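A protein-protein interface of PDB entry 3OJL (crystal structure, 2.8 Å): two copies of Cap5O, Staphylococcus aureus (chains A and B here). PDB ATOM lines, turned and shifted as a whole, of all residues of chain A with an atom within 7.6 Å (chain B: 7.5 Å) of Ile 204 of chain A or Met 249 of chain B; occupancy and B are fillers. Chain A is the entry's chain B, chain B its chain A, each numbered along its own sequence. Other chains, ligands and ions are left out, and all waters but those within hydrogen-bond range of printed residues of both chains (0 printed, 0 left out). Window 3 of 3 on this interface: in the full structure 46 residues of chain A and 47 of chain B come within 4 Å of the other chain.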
ATOM      1  N   HIS A 159     -23.748  32.163  19.397  1.00  0.00           N
ATOM      2  CA  HIS A 159     -23.292  31.132  18.491  1.00  0.00           C
ATOM      3  C   HIS A 159     -24.030  29.890  18.943  1.00  0.00           C
ATOM      4  O   HIS A 159     -23.936  29.496  20.109  1.00  0.00           O
ATOM      5  CB  HIS A 159     -21.775  30.941  18.542  1.00  0.00           C
ATOM      6  CG  HIS A 159     -21.287  29.736  17.788  1.00  0.00           C
ATOM      7  ND1 HIS A 159     -21.518  29.585  16.438  1.00  0.00           N
ATOM      8  CD2 HIS A 159     -20.571  28.681  18.225  1.00  0.00           C
ATOM      9  CE1 HIS A 159     -20.950  28.449  16.105  1.00  0.00           C
ATOM     10  NE2 HIS A 159     -20.355  27.879  17.145  1.00  0.00           N
ATOM     11  N   ARG A 163     -26.466  20.668  14.338  1.00  0.00           N
ATOM     12  CA  ARG A 163     -26.106  19.243  14.208  1.00  0.00           C
ATOM     13  C   ARG A 163     -27.312  18.637  13.491  1.00  0.00           C
ATOM     14  O   ARG A 163     -28.361  18.415  14.110  1.00  0.00           O
ATOM     15  CB  ARG A 163     -25.917  18.565  15.584  1.00  0.00           C
ATOM     16  CG  ARG A 163     -24.528  17.996  15.869  1.00  0.00           C
ATOM     17  CD  ARG A 163     -23.758  18.827  16.897  1.00  0.00           C
ATOM     18  NE  ARG A 163     -24.627  19.512  17.861  1.00  0.00           N
ATOM     19  CZ  ARG A 163     -24.216  20.402  18.761  1.00  0.00           C
ATOM     20  NH1 ARG A 163     -22.928  20.726  18.847  1.00  0.00           N
ATOM     21  NH2 ARG A 163     -25.088  20.976  19.582  1.00  0.00           N
ATOM     22  N   ASN A 176     -33.535  17.418  19.941  1.00  0.00           N
ATOM     23  CA  ASN A 176     -32.114  17.462  20.242  1.00  0.00           C
ATOM     24  C   ASN A 176     -31.723  18.566  21.204  1.00  0.00           C
ATOM     25  O   ASN A 176     -32.318  19.647  21.205  1.00  0.00           O
ATOM     26  CB  ASN A 176     -31.258  17.503  18.973  1.00  0.00           C
ATOM     27  CG  ASN A 176     -30.960  16.131  18.371  1.00  0.00           C
ATOM     28  OD1 ASN A 176     -31.650  15.124  18.612  1.00  0.00           O
ATOM     29  ND2 ASN A 176     -29.893  16.049  17.587  1.00  0.00           N
ATOM     30  N   ASN A 177     -30.717  18.265  22.038  1.00  0.00           N
ATOM     31  CA  ASN A 177     -30.124  19.190  22.985  1.00  0.00           C
ATOM     32  C   ASN A 177     -29.322  20.231  22.217  1.00  0.00           C
ATOM     33  O   ASN A 177     -28.578  19.889  21.286  1.00  0.00           O
ATOM     34  CB  ASN A 177     -29.239  18.446  23.981  1.00  0.00           C
ATOM     35  CG  ASN A 177     -30.035  17.670  24.989  1.00  0.00           C
ATOM     36  OD1 ASN A 177     -31.086  18.115  25.467  1.00  0.00           O
ATOM     37  ND2 ASN A 177     -29.548  16.486  25.329  1.00  0.00           N
ATOM     38  N   ARG A 178     -29.502  21.504  22.603  1.00  0.00           N
ATOM     39  CA  ARG A 178     -28.874  22.656  21.973  1.00  0.00           C
ATOM     40  C   ARG A 178     -27.912  23.352  22.885  1.00  0.00           C
ATOM     41  O   ARG A 178     -28.112  23.372  24.095  1.00  0.00           O
ATOM     42  CB  ARG A 178     -29.941  23.649  21.512  1.00  0.00           C
ATOM     43  CG  ARG A 178     -29.737  24.116  20.088  1.00  0.00           C
ATOM     44  CD  ARG A 178     -31.029  24.627  19.497  1.00  0.00           C
ATOM     45  NE  ARG A 178     -31.338  23.935  18.248  1.00  0.00           N
ATOM     46  CZ  ARG A 178     -31.956  22.756  18.167  1.00  0.00           C
ATOM     47  NH1 ARG A 178     -32.345  22.119  19.269  1.00  0.00           N
ATOM     48  NH2 ARG A 178     -32.179  22.199  16.988  1.00  0.00           N
ATOM     49  N   ILE A 179     -26.872  23.952  22.291  1.00  0.00           N
ATOM     50  CA  ILE A 179     -25.861  24.719  23.004  1.00  0.00           C
ATOM     51  C   ILE A 179     -26.085  26.192  22.669  1.00  0.00           C
ATOM     52  O   ILE A 179     -25.945  26.583  21.510  1.00  0.00           O
ATOM     53  CB  ILE A 179     -24.419  24.251  22.652  1.00  0.00           C
ATOM     54  CG1 ILE A 179     -24.234  22.718  22.883  1.00  0.00           C
ATOM     55  CG2 ILE A 179     -23.386  25.072  23.420  1.00  0.00           C
ATOM     56  CD1 ILE A 179     -23.028  22.038  22.135  1.00  0.00           C
ATOM     57  N   ILE A 180     -26.484  26.996  23.665  1.00  0.00           N
ATOM     58  CA  ILE A 180     -26.638  28.431  23.450  1.00  0.00           C
ATOM     59  C   ILE A 180     -25.339  29.043  23.979  1.00  0.00           C
ATOM     60  O   ILE A 180     -25.056  28.934  25.176  1.00  0.00           O
ATOM     61  CB  ILE A 180     -27.936  29.037  24.081  1.00  0.00           C
ATOM     62  CG1 ILE A 180     -29.216  28.178  23.814  1.00  0.00           C
ATOM     63  CG2 ILE A 180     -28.127  30.512  23.701  1.00  0.00           C
ATOM     64  CD1 ILE A 180     -29.736  28.087  22.413  1.00  0.00           C
ATOM     65  N   GLY A 181     -24.522  29.573  23.069  1.00  0.00           N
ATOM     66  CA  GLY A 181     -23.234  30.171  23.392  1.00  0.00           C
ATOM     67  C   GLY A 181     -23.281  31.662  23.201  1.00  0.00           C
ATOM     68  O   GLY A 181     -23.068  32.143  22.089  1.00  0.00           O
ATOM     69  N   GLY A 182     -23.624  32.384  24.257  1.00  0.00           N
ATOM     70  CA  GLY A 182     -23.753  33.832  24.206  1.00  0.00           C
ATOM     71  C   GLY A 182     -22.520  34.556  24.679  1.00  0.00           C
ATOM     72  O   GLY A 182     -21.856  34.100  25.609  1.00  0.00           O
ATOM     73  N   ILE A 188     -27.104  34.931  26.240  1.00  0.00           N
ATOM     74  CA  ILE A 188     -27.593  33.568  26.534  1.00  0.00           C
ATOM     75  C   ILE A 188     -29.134  33.584  26.672  1.00  0.00           C
ATOM     76  O   ILE A 188     -29.808  32.771  26.039  1.00  0.00           O
ATOM     77  CB  ILE A 188     -26.884  32.942  27.773  1.00  0.00           C
ATOM     78  CG1 ILE A 188     -25.378  32.744  27.517  1.00  0.00           C
ATOM     79  CG2 ILE A 188     -27.536  31.631  28.169  1.00  0.00           C
ATOM     80  CD1 ILE A 188     -24.509  32.614  28.753  1.00  0.00           C
ATOM     81  N   LYS A 192     -32.064  32.030  24.202  1.00  0.00           N
ATOM     82  CA  LYS A 192     -32.975  31.101  24.853  1.00  0.00           C
ATOM     83  C   LYS A 192     -34.430  31.470  24.514  1.00  0.00           C
ATOM     84  O   LYS A 192     -35.234  30.574  24.270  1.00  0.00           O
ATOM     85  CB  LYS A 192     -32.732  31.075  26.370  1.00  0.00           C
ATOM     86  CG  LYS A 192     -31.526  30.211  26.767  1.00  0.00           C
ATOM     87  CD  LYS A 192     -31.661  29.556  28.139  1.00  0.00           C
ATOM     88  CE  LYS A 192     -31.337  30.483  29.278  1.00  0.00           C
ATOM     89  NZ  LYS A 192     -31.825  29.938  30.566  1.00  0.00           N
ATOM     90  N   GLY A 201     -35.962  20.040  23.598  1.00  0.00           N
ATOM     91  CA  GLY A 201     -34.683  19.629  24.171  1.00  0.00           C
ATOM     92  C   GLY A 201     -34.109  20.618  25.171  1.00  0.00           C
ATOM     93  O   GLY A 201     -34.680  21.688  25.409  1.00  0.00           O
ATOM     94  N   GLU A 202     -32.972  20.261  25.774  1.00  0.00           N
ATOM     95  CA  GLU A 202     -32.307  21.090  26.771  1.00  0.00           C
ATOM     96  C   GLU A 202     -31.547  22.260  26.116  1.00  0.00           C
ATOM     97  O   GLU A 202     -31.002  22.108  25.022  1.00  0.00           O
ATOM     98  CB  GLU A 202     -31.388  20.224  27.661  1.00  0.00           C
ATOM     99  CG  GLU A 202     -30.870  20.884  28.930  1.00  0.00           C
ATOM    100  CD  GLU A 202     -31.894  21.025  30.039  1.00  0.00           C
ATOM    101  OE1 GLU A 202     -31.926  20.148  30.932  1.00  0.00           O
ATOM    102  OE2 GLU A 202     -32.674  22.006  30.006  1.00  0.00           O
ATOM    103  N   MET A 203     -31.550  23.429  26.784  1.00  0.00           N
ATOM    104  CA  MET A 203     -30.853  24.636  26.360  1.00  0.00           C
ATOM    105  C   MET A 203     -29.611  24.684  27.202  1.00  0.00           C
ATOM    106  O   MET A 203     -29.674  25.130  28.353  1.00  0.00           O
ATOM    107  CB  MET A 203     -31.683  25.899  26.645  1.00  0.00           C
ATOM    108  CG  MET A 203     -32.981  25.951  25.934  1.00  0.00           C
ATOM    109  SD  MET A 203     -32.789  26.474  24.227  1.00  0.00           S
ATOM    110  CE  MET A 203     -34.105  27.577  24.119  1.00  0.00           C
ATOM    111  N   ILE A 204     -28.488  24.191  26.658  1.00  0.00           N
ATOM    112  CA  ILE A 204     -27.223  24.179  27.372  1.00  0.00           C
ATOM    113  C   ILE A 204     -26.612  25.571  27.323  1.00  0.00           C
ATOM    114  O   ILE A 204     -26.158  26.011  26.267  1.00  0.00           O
ATOM    115  CB  ILE A 204     -26.254  23.056  26.936  1.00  0.00           C
ATOM    116  CG1 ILE A 204     -26.958  21.692  26.894  1.00  0.00           C
ATOM    117  CG2 ILE A 204     -25.079  23.008  27.887  1.00  0.00           C
ATOM    118  CD1 ILE A 204     -26.460  20.786  25.798  1.00  0.00           C
ATOM    119  N   GLU A 205     -26.635  26.269  28.474  1.00  0.00           N
ATOM    120  CA  GLU A 205     -26.100  27.617  28.645  1.00  0.00           C
ATOM    121  C   GLU A 205     -24.578  27.583  28.744  1.00  0.00           C
ATOM    122  O   GLU A 205     -24.025  26.808  29.540  1.00  0.00           O
ATOM    123  CB  GLU A 205     -26.694  28.279  29.900  1.00  0.00           C
ATOM    124  CG  GLU A 205     -28.210  28.414  29.874  1.00  0.00           C
ATOM    125  CD  GLU A 205     -28.858  28.723  31.209  1.00  0.00           C
ATOM    126  OE1 GLU A 205     -28.396  29.667  31.889  1.00  0.00           O
ATOM    127  OE2 GLU A 205     -29.864  28.057  31.551  1.00  0.00           O
ATOM    128  N   THR A 206     -23.907  28.416  27.920  1.00  0.00           N
ATOM    129  CA  THR A 206     -22.436  28.568  27.872  1.00  0.00           C
ATOM    130  C   THR A 206     -22.070  29.868  27.161  1.00  0.00           C
ATOM    131  O   THR A 206     -22.967  30.539  26.655  1.00  0.00           O
ATOM    132  CB  THR A 206     -21.728  27.317  27.266  1.00  0.00           C
ATOM    133  OG1 THR A 206     -20.338  27.434  27.475  1.00  0.00           O
ATOM    134  CG2 THR A 206     -21.959  27.155  25.786  1.00  0.00           C
ATOM    135  N   ASP A 207     -20.771  30.218  27.110  1.00  0.00           N
ATOM    136  CA  ASP A 207     -20.320  31.416  26.391  1.00  0.00           C
ATOM    137  C   ASP A 207     -19.919  31.050  24.959  1.00  0.00           C
ATOM    138  O   ASP A 207     -19.626  29.876  24.679  1.00  0.00           O
ATOM    139  CB  ASP A 207     -19.170  32.130  27.118  1.00  0.00           C
ATOM    140  CG  ASP A 207     -17.881  31.324  27.258  1.00  0.00           C
ATOM    141  OD1 ASP A 207     -17.810  30.213  26.724  1.00  0.00           O
ATOM    142  OD2 ASP A 207     -16.953  31.800  27.920  1.00  0.00           O
ATOM    143  N   THR A 210     -16.715  28.739  24.244  1.00  0.00           N
ATOM    144  CA  THR A 210     -16.910  27.334  24.637  1.00  0.00           C
ATOM    145  C   THR A 210     -17.792  26.627  23.615  1.00  0.00           C
ATOM    146  O   THR A 210     -17.422  25.534  23.194  1.00  0.00           O
ATOM    147  CB  THR A 210     -17.376  27.211  26.082  1.00  0.00           C
ATOM    148  OG1 THR A 210     -16.446  27.905  26.923  1.00  0.00           O
ATOM    149  CG2 THR A 210     -17.497  25.771  26.540  1.00  0.00           C
ATOM    150  N   ALA A 211     -18.909  27.264  23.151  1.00  0.00           N
ATOM    151  CA  ALA A 211     -19.800  26.708  22.120  1.00  0.00           C
ATOM    152  C   ALA A 211     -19.057  26.484  20.810  1.00  0.00           C
ATOM    153  O   ALA A 211     -19.227  25.443  20.201  1.00  0.00           O
ATOM    154  CB  ALA A 211     -20.999  27.615  21.897  1.00  0.00           C
ATOM    155  N   MET A 213     -15.544  26.217  20.359  1.00  0.00           N
ATOM    156  CA  MET A 213     -14.517  25.207  20.596  1.00  0.00           C
ATOM    157  C   MET A 213     -15.105  23.807  20.717  1.00  0.00           C
ATOM    158  O   MET A 213     -14.558  22.882  20.137  1.00  0.00           O
ATOM    159  CB  MET A 213     -13.594  25.599  21.774  1.00  0.00           C
ATOM    160  CG  MET A 213     -12.234  24.877  21.847  1.00  0.00           C
ATOM    161  SD  MET A 213     -11.370  24.654  20.260  1.00  0.00           S
ATOM    162  CE  MET A 213      -9.764  25.290  20.647  1.00  0.00           C
ATOM    163  N   SER A 214     -16.249  23.647  21.381  1.00  0.00           N
ATOM    164  CA  SER A 214     -16.820  22.309  21.500  1.00  0.00           C
ATOM    165  C   SER A 214     -17.245  21.674  20.201  1.00  0.00           C
ATOM    166  O   SER A 214     -16.960  20.497  20.032  1.00  0.00           O
ATOM    167  CB  SER A 214     -17.883  22.206  22.595  1.00  0.00           C
ATOM    168  OG  SER A 214     -19.147  22.688  22.185  1.00  0.00           O
ATOM    169  N   LYS A 215     -17.843  22.442  19.256  1.00  0.00           N
ATOM    170  CA  LYS A 215     -18.281  21.896  17.968  1.00  0.00           C
ATOM    171  C   LYS A 215     -17.093  21.414  17.170  1.00  0.00           C
ATOM    172  O   LYS A 215     -17.085  20.329  16.594  1.00  0.00           O
ATOM    173  CB  LYS A 215     -19.120  22.921  17.178  1.00  0.00           C
ATOM    174  CG  LYS A 215     -20.383  22.303  16.562  1.00  0.00           C
ATOM    175  CD  LYS A 215     -20.238  21.994  15.084  1.00  0.00           C
ATOM    176  CE  LYS A 215     -21.332  21.094  14.564  1.00  0.00           C
ATOM    177  NZ  LYS A 215     -21.075  19.670  14.905  1.00  0.00           N
ATOM    178  N   MET A 217     -14.179  20.514  18.555  1.00  0.00           N
ATOM    179  CA  MET A 217     -13.629  19.372  19.280  1.00  0.00           C
ATOM    180  C   MET A 217     -14.366  18.071  18.939  1.00  0.00           C
ATOM    181  O   MET A 217     -13.725  17.025  18.764  1.00  0.00           O
ATOM    182  CB  MET A 217     -13.666  19.627  20.782  1.00  0.00           C
ATOM    183  CG  MET A 217     -12.416  20.244  21.305  1.00  0.00           C
ATOM    184  SD  MET A 217     -12.428  20.125  23.125  1.00  0.00           S
ATOM    185  CE  MET A 217     -11.084  21.251  23.576  1.00  0.00           C
ATOM    186  N   GLU A 218     -15.708  18.159  18.796  1.00  0.00           N
ATOM    187  CA  GLU A 218     -16.586  17.065  18.406  1.00  0.00           C
ATOM    188  C   GLU A 218     -16.113  16.567  17.062  1.00  0.00           C
ATOM    189  O   GLU A 218     -16.077  15.364  16.857  1.00  0.00           O
ATOM    190  CB  GLU A 218     -18.044  17.542  18.277  1.00  0.00           C
ATOM    191  CG  GLU A 218     -18.810  17.726  19.578  1.00  0.00           C
ATOM    192  CD  GLU A 218     -20.223  18.253  19.418  1.00  0.00           C
ATOM    193  OE1 GLU A 218     -20.714  18.981  20.317  1.00  0.00           O
ATOM    194  OE2 GLU A 218     -20.837  17.935  18.374  1.00  0.00           O
ATOM    195  N   VAL B 243     -10.332  24.147  28.372  1.00  0.00           N
ATOM    196  CA  VAL B 243     -10.326  22.807  27.768  1.00  0.00           C
ATOM    197  C   VAL B 243     -11.308  21.852  28.476  1.00  0.00           C
ATOM    198  O   VAL B 243     -12.056  21.135  27.802  1.00  0.00           O
ATOM    199  CB  VAL B 243      -8.879  22.226  27.611  1.00  0.00           C
ATOM    200  CG1 VAL B 243      -8.195  22.016  28.961  1.00  0.00           C
ATOM    201  CG2 VAL B 243      -8.869  20.944  26.785  1.00  0.00           C
ATOM    202  N   LEU B 244     -11.338  21.887  29.819  1.00  0.00           N
ATOM    203  CA  LEU B 244     -12.175  20.994  30.627  1.00  0.00           C
ATOM    204  C   LEU B 244     -13.666  21.194  30.422  1.00  0.00           C
ATOM    205  O   LEU B 244     -14.407  20.210  30.296  1.00  0.00           O
ATOM    206  CB  LEU B 244     -11.772  21.036  32.098  1.00  0.00           C
ATOM    207  CG  LEU B 244     -10.284  20.791  32.362  1.00  0.00           C
ATOM    208  CD1 LEU B 244      -9.914  21.189  33.750  1.00  0.00           C
ATOM    209  CD2 LEU B 244      -9.893  19.351  32.093  1.00  0.00           C
ATOM    210  N   ASP B 245     -14.094  22.467  30.324  1.00  0.00           N
ATOM    211  CA  ASP B 245     -15.479  22.855  30.053  1.00  0.00           C
ATOM    212  C   ASP B 245     -15.848  22.442  28.629  1.00  0.00           C
ATOM    213  O   ASP B 245     -16.941  21.922  28.408  1.00  0.00           O
ATOM    214  CB  ASP B 245     -15.653  24.379  30.242  1.00  0.00           C
ATOM    215  CG  ASP B 245     -15.631  24.867  31.678  1.00  0.00           C
ATOM    216  OD1 ASP B 245     -16.000  24.071  32.593  1.00  0.00           O
ATOM    217  OD2 ASP B 245     -15.306  26.059  31.891  1.00  0.00           O
ATOM    218  N   VAL B 246     -14.913  22.647  27.678  1.00  0.00           N
ATOM    219  CA  VAL B 246     -15.065  22.270  26.272  1.00  0.00           C
ATOM    220  C   VAL B 246     -15.261  20.741  26.142  1.00  0.00           C
ATOM    221  O   VAL B 246     -16.218  20.334  25.476  1.00  0.00           O
ATOM    222  CB  VAL B 246     -13.935  22.818  25.360  1.00  0.00           C
ATOM    223  CG1 VAL B 246     -14.165  22.390  23.940  1.00  0.00           C
ATOM    224  CG2 VAL B 246     -13.869  24.340  25.402  1.00  0.00           C
ATOM    225  N   ILE B 247     -14.383  19.905  26.789  1.00  0.00           N
ATOM    226  CA  ILE B 247     -14.480  18.428  26.772  1.00  0.00           C
ATOM    227  C   ILE B 247     -15.867  17.960  27.269  1.00  0.00           C
ATOM    228  O   ILE B 247     -16.483  17.113  26.620  1.00  0.00           O
ATOM    229  CB  ILE B 247     -13.286  17.723  27.518  1.00  0.00           C
ATOM    230  CG1 ILE B 247     -11.973  17.899  26.716  1.00  0.00           C
ATOM    231  CG2 ILE B 247     -13.562  16.224  27.812  1.00  0.00           C
ATOM    232  CD1 ILE B 247     -10.664  17.701  27.498  1.00  0.00           C
ATOM    233  N   GLU B 248     -16.362  18.542  28.393  1.00  0.00           N
ATOM    234  CA  GLU B 248     -17.656  18.214  28.991  1.00  0.00           C
ATOM    235  C   GLU B 248     -18.827  18.507  28.030  1.00  0.00           C
ATOM    236  O   GLU B 248     -19.772  17.714  27.952  1.00  0.00           O
ATOM    237  CB  GLU B 248     -17.830  18.956  30.323  1.00  0.00           C
ATOM    238  CG  GLU B 248     -18.819  18.290  31.272  1.00  0.00           C
ATOM    239  CD  GLU B 248     -19.803  19.202  31.986  1.00  0.00           C
ATOM    240  OE1 GLU B 248     -20.878  18.702  32.397  1.00  0.00           O
ATOM    241  OE2 GLU B 248     -19.506  20.411  32.134  1.00  0.00           O
ATOM    242  N   MET B 249     -18.747  19.634  27.294  1.00  0.00           N
ATOM    243  CA  MET B 249     -19.740  20.075  26.314  1.00  0.00           C
ATOM    244  C   MET B 249     -19.815  19.139  25.140  1.00  0.00           C
ATOM    245  O   MET B 249     -20.874  18.625  24.846  1.00  0.00           O
ATOM    246  CB  MET B 249     -19.394  21.467  25.787  1.00  0.00           C
ATOM    247  CG  MET B 249     -19.757  22.591  26.713  1.00  0.00           C
ATOM    248  SD  MET B 249     -21.512  22.700  27.083  1.00  0.00           S
ATOM    249  CE  MET B 249     -22.163  22.708  25.519  1.00  0.00           C
ATOM    250  N   ALA B 250     -18.692  18.949  24.447  1.00  0.00           N
ATOM    251  CA  ALA B 250     -18.541  18.099  23.275  1.00  0.00           C
ATOM    252  C   ALA B 250     -18.878  16.642  23.580  1.00  0.00           C
ATOM    253  O   ALA B 250     -19.441  15.965  22.723  1.00  0.00           O
ATOM    254  CB  ALA B 250     -17.117  18.215  22.741  1.00  0.00           C
ATOM    255  N   ASN B 251     -18.570  16.160  24.810  1.00  0.00           N
ATOM    256  CA  ASN B 251     -18.860  14.786  25.219  1.00  0.00           C
ATOM    257  C   ASN B 251     -20.363  14.459  25.416  1.00  0.00           C
ATOM    258  O   ASN B 251     -20.746  13.273  25.497  1.00  0.00           O
ATOM    259  CB  ASN B 251     -18.003  14.385  26.391  1.00  0.00           C
ATOM    260  CG  ASN B 251     -16.594  14.023  26.010  1.00  0.00           C
ATOM    261  OD1 ASN B 251     -16.205  14.028  24.839  1.00  0.00           O
ATOM    262  ND2 ASN B 251     -15.810  13.657  26.999  1.00  0.00           N
ATOM    263  N   LYS B 252     -21.212  15.513  25.407  1.00  0.00           N
ATOM    264  CA  LYS B 252     -22.657  15.427  25.478  1.00  0.00           C
ATOM    265  C   LYS B 252     -23.167  14.756  24.205  1.00  0.00           C
ATOM    266  O   LYS B 252     -24.239  14.176  24.206  1.00  0.00           O
ATOM    267  CB  LYS B 252     -23.272  16.815  25.689  1.00  0.00           C
ATOM    268  CG  LYS B 252     -22.909  17.433  27.033  1.00  0.00           C
ATOM    269  CD  LYS B 252     -23.686  18.705  27.314  1.00  0.00           C
ATOM    270  CE  LYS B 252     -23.130  19.435  28.514  1.00  0.00           C
ATOM    271  NZ  LYS B 252     -23.241  18.643  29.773  1.00  0.00           N
ATOM    272  N   HIS B 253     -22.370  14.784  23.128  1.00  0.00           N
ATOM    273  CA  HIS B 253     -22.664  14.085  21.881  1.00  0.00           C
ATOM    274  C   HIS B 253     -22.434  12.560  22.142  1.00  0.00           C
ATOM    275  O   HIS B 253     -21.425  12.177  22.742  1.00  0.00           O
ATOM    276  CB  HIS B 253     -21.763  14.605  20.749  1.00  0.00           C
ATOM    277  CG  HIS B 253     -22.126  14.080  19.401  1.00  0.00           C
ATOM    278  ND1 HIS B 253     -22.560  14.914  18.397  1.00  0.00           N
ATOM    279  CD2 HIS B 253     -22.075  12.818  18.924  1.00  0.00           C
ATOM    280  CE1 HIS B 253     -22.775  14.141  17.351  1.00  0.00           C
ATOM    281  NE2 HIS B 253     -22.510  12.866  17.629  1.00  0.00           N
ATOM    282  N   VAL B 256     -19.117  11.086  20.624  1.00  0.00           N
ATOM    283  CA  VAL B 256     -17.920  11.830  21.059  1.00  0.00           C
ATOM    284  C   VAL B 256     -17.571  11.478  22.531  1.00  0.00           C
ATOM    285  O   VAL B 256     -18.407  11.598  23.434  1.00  0.00           O
ATOM    286  CB  VAL B 256     -18.074  13.348  20.814  1.00  0.00           C
ATOM    287  CG1 VAL B 256     -16.842  14.109  21.286  1.00  0.00           C
ATOM    288  CG2 VAL B 256     -18.343  13.646  19.346  1.00  0.00           C
ATOM    289  N   ILE B 258     -14.159  12.310  24.152  1.00  0.00           N
ATOM    290  CA  ILE B 258     -12.863  12.960  24.365  1.00  0.00           C
ATOM    291  C   ILE B 258     -12.372  12.604  25.735  1.00  0.00           C
ATOM    292  O   ILE B 258     -13.150  12.647  26.677  1.00  0.00           O
ATOM    293  CB  ILE B 258     -12.900  14.497  24.128  1.00  0.00           C
ATOM    294  CG1 ILE B 258     -13.347  14.822  22.688  1.00  0.00           C
ATOM    295  CG2 ILE B 258     -11.540  15.159  24.435  1.00  0.00           C
ATOM    296  CD1 ILE B 258     -14.075  16.199  22.545  1.00  0.00           C
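Ile 204 of chain A touches Met 249 of chain B.
Met 249 of chain B touches Thr 210 of chain A (CG to CG2, 3.9 Å).
C of Met 213 of chain A touches CG1 of Val 246 of chain B, at 3.6 Å.
CG1 of Val 246 of chain B touches N of Ser 214 of chain A, at 3.5 Å.
CB of Met 249 of chain B touches CB of Ser 214 of chain A (3.6 Å).
CB of Ala 250 of chain B touches O of Ser 214 of chain A, 3.5 Å away.
Met 217 of chain A touches Val 243 of chain B (CE to CG2, 3.9 Å).
CG1 of Val 246 of chain B touches SD of Met 217 of chain A, at 3.0 Å.
Met 217 of chain A touches Ile 258 of chain B (CB to CD1, 3.9 Å).
Glu 218 of chain A touches Val 256 of chain B.
ND1 of His 253 of chain B sits at hydrogen-bond distance from OE2 of Glu 218 of chain A (3.5 Å).
N of Ile 180 of chain A is in hydrogen-bond range of O of Ile 204 of chain A (2.8 Å).
OD1 of Asp 207 of chain A sits at hydrogen-bond distance from OG1 of Thr 210 of chain A.
The side-chain hydroxyl (OG) of Ser 214 of chain A is in hydrogen-bond range of the backbone carbonyl oxygen (O) of Ala 211 of chain A, at 3.4 Å.
The side-chain amino group (NZ) of Lys 215 of chain A is in salt-bridge range of the side-chain carboxylate (OE2) of Glu 218 of chain A, at 3.9 Å.
The side-chain carboxylate (OE1) of Glu 218 of chain A lies within salt-bridge range of the guanidinium group (NH1) of Arg 163 of chain A (3.2 Å).
The backbone carbonyl oxygen (O) of Thr 210 of chain A lies close to the side-chain hydroxyl (OG) of Ser 214 of chain A, 3.5 Å away.
Ile 204 of chain A touches just these residues of chain B: Met 249 (3.7 Å) and Lys 252 (3.8 Å).
Printed residues of chain B within 4 Å of Thr 210 of chain A: Met 249 (3.9 Å).
Of the printed residues of chain B, Met 213 of chain A touches Val 246 (3.6 Å).
Printed residues of chain B within 4 Å of Met 217 of chain A: Val 243, Val 246 and Ile 258.
Of the printed residues of chain B, Glu 218 of chain A touches Ala 250, His 253 and Val 256.
Met 249 of chain B touches just these residues of chain A: Ile 179 (3.4 Å), Ile 204 (3.7 Å), Thr 210 (3.9 Å) and Ser 214 (3.6 Å).
Of the printed residues of chain A, Val 256 of chain B touches Glu 218.
The nearest residue of chain A that does not touch Met 249 of chain B is Thr 206 of chain A (4.5 Å).
No position is printed for both chains.
Hydrophobic or aromatic side chains of chain B within 4 Å of the printed part of chain A: Val 243, Val 246, Met 249, Ala 250, His 253, Val 256 and Ile 258.
Hydrophobic or aromatic side chains of chain A that line the printed part of chain B: Ile 179, Ile 204, Met 213 and Met 217.
Among the printed residues, 14 pairs touch across the chains.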
